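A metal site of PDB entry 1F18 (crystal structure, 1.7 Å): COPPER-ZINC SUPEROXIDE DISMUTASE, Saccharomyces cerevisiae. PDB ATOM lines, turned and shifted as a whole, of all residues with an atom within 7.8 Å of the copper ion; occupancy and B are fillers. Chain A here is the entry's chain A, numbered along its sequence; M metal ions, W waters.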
ATOM      1  N   GLY A  45     -25.776 -19.344   0.358  1.00  0.00           N
ATOM      2  CA  GLY A  45     -26.666 -19.745  -0.736  1.00  0.00           C
ATOM      3  C   GLY A  45     -25.893 -20.061  -1.988  1.00  0.00           C
ATOM      4  O   GLY A  45     -24.972 -19.332  -2.369  1.00  0.00           O
ATOM      5  N   PHE A  46     -26.313 -21.099  -2.706  1.00  0.00           N
ATOM      6  CA  PHE A  46     -25.561 -21.578  -3.866  1.00  0.00           C
ATOM      7  C   PHE A  46     -26.600 -22.095  -4.869  1.00  0.00           C
ATOM      8  O   PHE A  46     -27.286 -23.078  -4.588  1.00  0.00           O
ATOM      9  CB  PHE A  46     -24.667 -22.697  -3.294  1.00  0.00           C
ATOM     10  CG  PHE A  46     -23.764 -23.364  -4.283  1.00  0.00           C
ATOM     11  CD1 PHE A  46     -22.850 -22.643  -5.041  1.00  0.00           C
ATOM     12  CD2 PHE A  46     -23.759 -24.764  -4.399  1.00  0.00           C
ATOM     13  CE1 PHE A  46     -21.961 -23.287  -5.897  1.00  0.00           C
ATOM     14  CE2 PHE A  46     -22.867 -25.427  -5.255  1.00  0.00           C
ATOM     15  CZ  PHE A  46     -21.961 -24.687  -6.005  1.00  0.00           C
ATOM     16  N   HIS A  47     -26.726 -21.436  -6.030  1.00  0.00           N
ATOM     17  CA  HIS A  47     -27.762 -21.839  -7.000  1.00  0.00           C
ATOM     18  C   HIS A  47     -27.365 -21.756  -8.461  1.00  0.00           C
ATOM     19  O   HIS A  47     -26.434 -21.066  -8.826  1.00  0.00           O
ATOM     20  CB  HIS A  47     -29.015 -20.900  -6.901  1.00  0.00           C
ATOM     21  CG  HIS A  47     -29.383 -20.491  -5.506  1.00  0.00           C
ATOM     22  ND1 HIS A  47     -29.219 -19.207  -5.040  1.00  0.00           N
ATOM     23  CD2 HIS A  47     -29.871 -21.211  -4.470  1.00  0.00           C
ATOM     24  CE1 HIS A  47     -29.578 -19.148  -3.769  1.00  0.00           C
ATOM     25  NE2 HIS A  47     -29.981 -20.349  -3.404  1.00  0.00           N
ATOM     26  N   ILE A  48     -28.176 -22.406  -9.303  1.00  0.00           N
ATOM     27  CA  ILE A  48     -28.040 -22.301 -10.754  1.00  0.00           C
ATOM     28  C   ILE A  48     -29.058 -21.186 -11.120  1.00  0.00           C
ATOM     29  O   ILE A  48     -30.210 -21.201 -10.653  1.00  0.00           O
ATOM     30  CB  ILE A  48     -28.474 -23.570 -11.543  1.00  0.00           C
ATOM     31  CG1 ILE A  48     -27.765 -24.807 -10.996  1.00  0.00           C
ATOM     32  CG2 ILE A  48     -28.244 -23.347 -13.034  1.00  0.00           C
ATOM     33  CD1 ILE A  48     -26.288 -24.736 -11.138  1.00  0.00           C
ATOM     34  N   HIS A  49     -28.552 -20.162 -11.786  1.00  0.00           N
ATOM     35  CA  HIS A  49     -29.368 -19.043 -12.252  1.00  0.00           C
ATOM     36  C   HIS A  49     -29.664 -19.237 -13.748  1.00  0.00           C
ATOM     37  O   HIS A  49     -28.923 -19.932 -14.462  1.00  0.00           O
ATOM     38  CB  HIS A  49     -28.721 -17.694 -11.937  1.00  0.00           C
ATOM     39  CG  HIS A  49     -28.835 -17.316 -10.499  1.00  0.00           C
ATOM     40  ND1 HIS A  49     -29.393 -16.130 -10.084  1.00  0.00           N
ATOM     41  CD2 HIS A  49     -28.467 -17.982  -9.381  1.00  0.00           C
ATOM     42  CE1 HIS A  49     -29.345 -16.073  -8.758  1.00  0.00           C
ATOM     43  NE2 HIS A  49     -28.779 -17.189  -8.312  1.00  0.00           N
ATOM     44  N   GLY A  62     -29.657 -13.298 -14.034  1.00  0.00           N
ATOM     45  CA  GLY A  62     -31.079 -13.449 -13.876  1.00  0.00           C
ATOM     46  C   GLY A  62     -31.462 -14.127 -12.577  1.00  0.00           C
ATOM     47  O   GLY A  62     -30.663 -14.219 -11.630  1.00  0.00           O
ATOM     48  N   PRO A  63     -32.698 -14.643 -12.497  1.00  0.00           N
ATOM     49  CA  PRO A  63     -33.230 -15.313 -11.310  1.00  0.00           C
ATOM     50  C   PRO A  63     -32.804 -16.811 -11.300  1.00  0.00           C
ATOM     51  O   PRO A  63     -32.121 -17.292 -12.209  1.00  0.00           O
ATOM     52  CB  PRO A  63     -34.738 -15.130 -11.519  1.00  0.00           C
ATOM     53  CG  PRO A  63     -34.839 -15.407 -12.974  1.00  0.00           C
ATOM     54  CD  PRO A  63     -33.703 -14.638 -13.585  1.00  0.00           C
ATOM     55  N   HIS A  64     -33.194 -17.522 -10.252  1.00  0.00           N
ATOM     56  CA  HIS A  64     -32.892 -18.958 -10.159  1.00  0.00           C
ATOM     57  C   HIS A  64     -33.544 -19.684 -11.332  1.00  0.00           C
ATOM     58  O   HIS A  64     -34.662 -19.334 -11.752  1.00  0.00           O
ATOM     59  CB  HIS A  64     -33.463 -19.530  -8.883  1.00  0.00           C
ATOM     60  CG  HIS A  64     -32.870 -18.955  -7.639  1.00  0.00           C
ATOM     61  ND1 HIS A  64     -33.306 -19.319  -6.385  1.00  0.00           N
ATOM     62  CD2 HIS A  64     -31.900 -18.019  -7.452  1.00  0.00           C
ATOM     63  CE1 HIS A  64     -32.647 -18.623  -5.467  1.00  0.00           C
ATOM     64  NE2 HIS A  64     -31.794 -17.827  -6.093  1.00  0.00           N
ATOM     65  N   PHE A  65     -32.810 -20.659 -11.895  1.00  0.00           N
ATOM     66  CA  PHE A  65     -33.311 -21.456 -13.017  1.00  0.00           C
ATOM     67  C   PHE A  65     -34.560 -22.199 -12.483  1.00  0.00           C
ATOM     68  O   PHE A  65     -34.500 -22.981 -11.522  1.00  0.00           O
ATOM     69  CB  PHE A  65     -32.208 -22.379 -13.520  1.00  0.00           C
ATOM     70  CG  PHE A  65     -32.609 -23.211 -14.715  1.00  0.00           C
ATOM     71  CD1 PHE A  65     -33.314 -22.647 -15.771  1.00  0.00           C
ATOM     72  CD2 PHE A  65     -32.314 -24.583 -14.750  1.00  0.00           C
ATOM     73  CE1 PHE A  65     -33.728 -23.456 -16.855  1.00  0.00           C
ATOM     74  CE2 PHE A  65     -32.724 -25.370 -15.829  1.00  0.00           C
ATOM     75  CZ  PHE A  65     -33.433 -24.807 -16.877  1.00  0.00           C
ATOM     76  N   HIS A  72     -39.190 -21.276  -4.404  1.00  0.00           N
ATOM     77  CA  HIS A  72     -37.842 -21.578  -3.890  1.00  0.00           C
ATOM     78  C   HIS A  72     -37.915 -22.568  -2.696  1.00  0.00           C
ATOM     79  O   HIS A  72     -38.705 -22.371  -1.765  1.00  0.00           O
ATOM     80  CB  HIS A  72     -37.200 -20.254  -3.440  1.00  0.00           C
ATOM     81  CG  HIS A  72     -35.810 -20.428  -2.962  1.00  0.00           C
ATOM     82  ND1 HIS A  72     -34.759 -20.674  -3.835  1.00  0.00           N
ATOM     83  CD2 HIS A  72     -35.301 -20.501  -1.720  1.00  0.00           C
ATOM     84  CE1 HIS A  72     -33.669 -20.904  -3.120  1.00  0.00           C
ATOM     85  NE2 HIS A  72     -33.973 -20.804  -1.837  1.00  0.00           N
ATOM     86  N   GLY A  83     -32.710 -25.010 -10.025  1.00  0.00           N
ATOM     87  CA  GLY A  83     -31.420 -24.481  -9.594  1.00  0.00           C
ATOM     88  C   GLY A  83     -31.134 -24.402  -8.101  1.00  0.00           C
ATOM     89  O   GLY A  83     -30.062 -23.948  -7.734  1.00  0.00           O
ATOM     90  N   ASP A  84     -32.041 -24.842  -7.237  1.00  0.00           N
ATOM     91  CA  ASP A  84     -31.845 -24.792  -5.800  1.00  0.00           C
ATOM     92  C   ASP A  84     -30.878 -25.837  -5.238  1.00  0.00           C
ATOM     93  O   ASP A  84     -31.209 -27.005  -5.119  1.00  0.00           O
ATOM     94  CB  ASP A  84     -33.193 -24.884  -5.081  1.00  0.00           C
ATOM     95  CG  ASP A  84     -34.046 -23.649  -5.294  1.00  0.00           C
ATOM     96  OD1 ASP A  84     -33.488 -22.670  -5.815  1.00  0.00           O
ATOM     97  OD2 ASP A  84     -35.252 -23.628  -4.926  1.00  0.00           O
ATOM     98  N   SER A 117     -25.824 -20.211 -15.400  1.00  0.00           N
ATOM     99  CA  SER A 117     -24.819 -19.713 -14.452  1.00  0.00           C
ATOM    100  C   SER A 117     -24.929 -20.295 -13.089  1.00  0.00           C
ATOM    101  O   SER A 117     -25.985 -20.733 -12.686  1.00  0.00           O
ATOM    102  CB  SER A 117     -24.949 -18.180 -14.237  1.00  0.00           C
ATOM    103  OG  SER A 117     -24.515 -17.433 -15.349  1.00  0.00           O
ATOM    104  N   VAL A 118     -23.810 -20.296 -12.364  1.00  0.00           N
ATOM    105  CA  VAL A 118     -23.800 -20.711 -10.964  1.00  0.00           C
ATOM    106  C   VAL A 118     -23.501 -19.409 -10.219  1.00  0.00           C
ATOM    107  O   VAL A 118     -22.643 -18.643 -10.646  1.00  0.00           O
ATOM    108  CB  VAL A 118     -22.630 -21.694 -10.580  1.00  0.00           C
ATOM    109  CG1 VAL A 118     -22.717 -21.971  -9.089  1.00  0.00           C
ATOM    110  CG2 VAL A 118     -22.695 -22.993 -11.339  1.00  0.00           C
ATOM    111  N   VAL A 119     -24.214 -19.170  -9.135  1.00  0.00           N
ATOM    112  CA  VAL A 119     -24.014 -18.015  -8.271  1.00  0.00           C
ATOM    113  C   VAL A 119     -23.820 -18.443  -6.798  1.00  0.00           C
ATOM    114  O   VAL A 119     -24.546 -19.311  -6.276  1.00  0.00           O
ATOM    115  CB  VAL A 119     -25.196 -17.029  -8.324  1.00  0.00           C
ATOM    116  CG1 VAL A 119     -25.044 -15.944  -7.261  1.00  0.00           C
ATOM    117  CG2 VAL A 119     -25.293 -16.426  -9.727  1.00  0.00           C
ATOM    118  N   ILE A 120     -22.759 -17.909  -6.188  1.00  0.00           N
ATOM    119  CA  ILE A 120     -22.460 -18.125  -4.766  1.00  0.00           C
ATOM    120  C   ILE A 120     -22.878 -16.799  -4.084  1.00  0.00           C
ATOM    121  O   ILE A 120     -22.484 -15.726  -4.544  1.00  0.00           O
ATOM    122  CB  ILE A 120     -20.939 -18.497  -4.492  1.00  0.00           C
ATOM    123  CG1 ILE A 120     -20.703 -18.672  -3.000  1.00  0.00           C
ATOM    124  CG2 ILE A 120     -19.951 -17.480  -5.104  1.00  0.00           C
ATOM    125  CD1 ILE A 120     -21.441 -19.844  -2.389  1.00  0.00           C
ATOM    126  N   HIS A 121     -23.688 -16.897  -3.034  1.00  0.00           N
ATOM    127  CA  HIS A 121     -24.205 -15.740  -2.305  1.00  0.00           C
ATOM    128  C   HIS A 121     -23.434 -15.316  -1.083  1.00  0.00           C
ATOM    129  O   HIS A 121     -22.686 -16.106  -0.506  1.00  0.00           O
ATOM    130  CB  HIS A 121     -25.672 -15.970  -1.889  1.00  0.00           C
ATOM    131  CG  HIS A 121     -26.603 -15.964  -3.060  1.00  0.00           C
ATOM    132  ND1 HIS A 121     -27.152 -14.796  -3.552  1.00  0.00           N
ATOM    133  CD2 HIS A 121     -26.948 -16.933  -3.927  1.00  0.00           C
ATOM    134  CE1 HIS A 121     -27.775 -15.046  -4.686  1.00  0.00           C
ATOM    135  NE2 HIS A 121     -27.661 -16.339  -4.941  1.00  0.00           N
ATOM    136  N   ASP A 125     -29.106 -19.038   2.699  1.00  0.00           N
ATOM    137  CA  ASP A 125     -30.384 -19.290   2.013  1.00  0.00           C
ATOM    138  C   ASP A 125     -31.341 -19.905   3.057  1.00  0.00           C
ATOM    139  O   ASP A 125     -31.008 -20.925   3.675  1.00  0.00           O
ATOM    140  CB  ASP A 125     -30.099 -20.244   0.870  1.00  0.00           C
ATOM    141  CG  ASP A 125     -31.333 -20.657   0.072  1.00  0.00           C
ATOM    142  OD1 ASP A 125     -32.496 -20.550   0.553  1.00  0.00           O
ATOM    143  OD2 ASP A 125     -31.109 -21.133  -1.064  1.00  0.00           O
ATOM    144  N   LYS A 137     -38.764 -16.705  -3.310  1.00  0.00           N
ATOM    145  CA  LYS A 137     -38.162 -16.341  -4.582  1.00  0.00           C
ATOM    146  C   LYS A 137     -36.676 -16.611  -4.637  1.00  0.00           C
ATOM    147  O   LYS A 137     -36.157 -17.148  -5.648  1.00  0.00           O
ATOM    148  CB  LYS A 137     -38.433 -14.839  -4.943  1.00  0.00           C
ATOM    149  CG  LYS A 137     -39.902 -14.439  -4.787  1.00  0.00           C
ATOM    150  CD  LYS A 137     -40.417 -13.494  -5.880  1.00  0.00           C
ATOM    151  CE  LYS A 137     -40.222 -12.009  -5.615  1.00  0.00           C
ATOM    152  NZ  LYS A 137     -41.166 -11.209  -6.518  1.00  0.00           N
ATOM    153  N   THR A 138     -35.976 -16.157  -3.583  1.00  0.00           N
ATOM    154  CA  THR A 138     -34.509 -16.262  -3.509  1.00  0.00           C
ATOM    155  C   THR A 138     -33.972 -16.930  -2.257  1.00  0.00           C
ATOM    156  O   THR A 138     -32.798 -17.203  -2.171  1.00  0.00           O
ATOM    157  CB  THR A 138     -33.863 -14.837  -3.551  1.00  0.00           C
ATOM    158  OG1 THR A 138     -34.293 -14.074  -2.414  1.00  0.00           O
ATOM    159  CG2 THR A 138     -34.255 -14.090  -4.794  1.00  0.00           C
ATOM    160  N   ALA A 141     -31.083 -15.101   0.207  1.00  0.00           N
ATOM    161  CA  ALA A 141     -29.654 -15.413   0.162  1.00  0.00           C
ATOM    162  C   ALA A 141     -28.751 -14.168   0.017  1.00  0.00           C
ATOM    163  O   ALA A 141     -27.519 -14.252   0.196  1.00  0.00           O
ATOM    164  CB  ALA A 141     -29.364 -16.456  -0.938  1.00  0.00           C
ATOM    165  N   GLY A 142     -29.366 -13.037  -0.353  1.00  0.00           N
ATOM    166  CA  GLY A 142     -28.613 -11.788  -0.449  1.00  0.00           C
ATOM    167  C   GLY A 142     -27.762 -11.548  -1.674  1.00  0.00           C
ATOM    168  O   GLY A 142     -28.019 -12.122  -2.729  1.00  0.00           O
ATOM    169  N   PRO A 143     -26.684 -10.727  -1.547  1.00  0.00           N
ATOM    170  CA  PRO A 143     -25.803 -10.416  -2.691  1.00  0.00           C
ATOM    171  C   PRO A 143     -25.137 -11.604  -3.379  1.00  0.00           C
ATOM    172  O   PRO A 143     -25.048 -12.683  -2.830  1.00  0.00           O
ATOM    173  CB  PRO A 143     -24.768  -9.460  -2.091  1.00  0.00           C
ATOM    174  CG  PRO A 143     -25.493  -8.870  -0.838  1.00  0.00           C
ATOM    175  CD  PRO A 143     -26.258 -10.041  -0.302  1.00  0.00           C
ATOM    176  N   ARG A 144     -24.613 -11.343  -4.565  1.00  0.00           N
ATOM    177  CA  ARG A 144     -23.954 -12.315  -5.417  1.00  0.00           C
ATOM    178  C   ARG A 144     -22.487 -11.903  -5.623  1.00  0.00           C
ATOM    179  O   ARG A 144     -22.117 -11.402  -6.721  1.00  0.00           O
ATOM    180  CB  ARG A 144     -24.649 -12.355  -6.801  1.00  0.00           C
ATOM    181  CG  ARG A 144     -26.163 -12.498  -6.768  1.00  0.00           C
ATOM    182  CD  ARG A 144     -26.740 -12.325  -8.208  1.00  0.00           C
ATOM    183  NE  ARG A 144     -28.195 -12.467  -8.174  1.00  0.00           N
ATOM    184  CZ  ARG A 144     -28.973 -12.631  -9.243  1.00  0.00           C
ATOM    185  NH1 ARG A 144     -28.475 -12.662 -10.476  1.00  0.00           N
ATOM    186  NH2 ARG A 144     -30.276 -12.798  -9.040  1.00  0.00           N
HETATM  187 CU    CU M   1     -28.763 -17.585  -6.266  1.00  0.00          CU
HETATM  188 ZN    ZN M   2     -34.437 -20.842  -5.788  1.00  0.00          ZN
HETATM  189  O   HOH W   1     -30.831 -15.971  -3.958  1.00  0.00           O
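NE2 of His 64 lies close to ND1 of His 47 (3.1 Å).
The backbone NH (N) of Val 119 sits at hydrogen-bond distance from the backbone carbonyl oxygen (O) of His 47 (2.9 Å).
NE2 of His 47 lies within hydrogen-bond range of OD2 of Asp 125, 2.7 Å away.
ND1 of His 49 sits at hydrogen-bond distance from O of Gly 62 (2.8 Å).
The backbone carbonyl oxygen of Ser 117 is in hydrogen-bond range of the backbone NH of His 49 (2.8 Å).
The backbone NH (N) of His 121 sits at hydrogen-bond distance from the backbone carbonyl oxygen (O) of Gly 45 (2.8 Å).
A ring nitrogen (ND1) of His 121 sits at hydrogen-bond distance from the backbone carbonyl oxygen of Gly 142, 2.9 Å away.
The backbone carbonyl oxygen (O) of Pro 143 is in hydrogen-bond range of a ring nitrogen (ND1) of His 121 (3.1 Å).
Merely in contact with the copper ion: His 64 (3.0 Å).
Four residues have an atom within 4 Å of the copper ion: His 47, His 49, His 64 and His 121.
The nearest printed residue that does not touch the copper ion is Val 119 (4.2 Å).
The copper ion is bound by a ring nitrogen (ND1) of His 47 (2.1 Å), a ring nitrogen (NE2) of His 49 (2.1 Å) and a ring nitrogen (NE2) of His 121 (2.1 Å).
The copper ion has three donor atoms within binding distance.
Water W1 bridges O of Thr 138 (2.9 Å) and NE2 of His 64 (3.0 Å).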
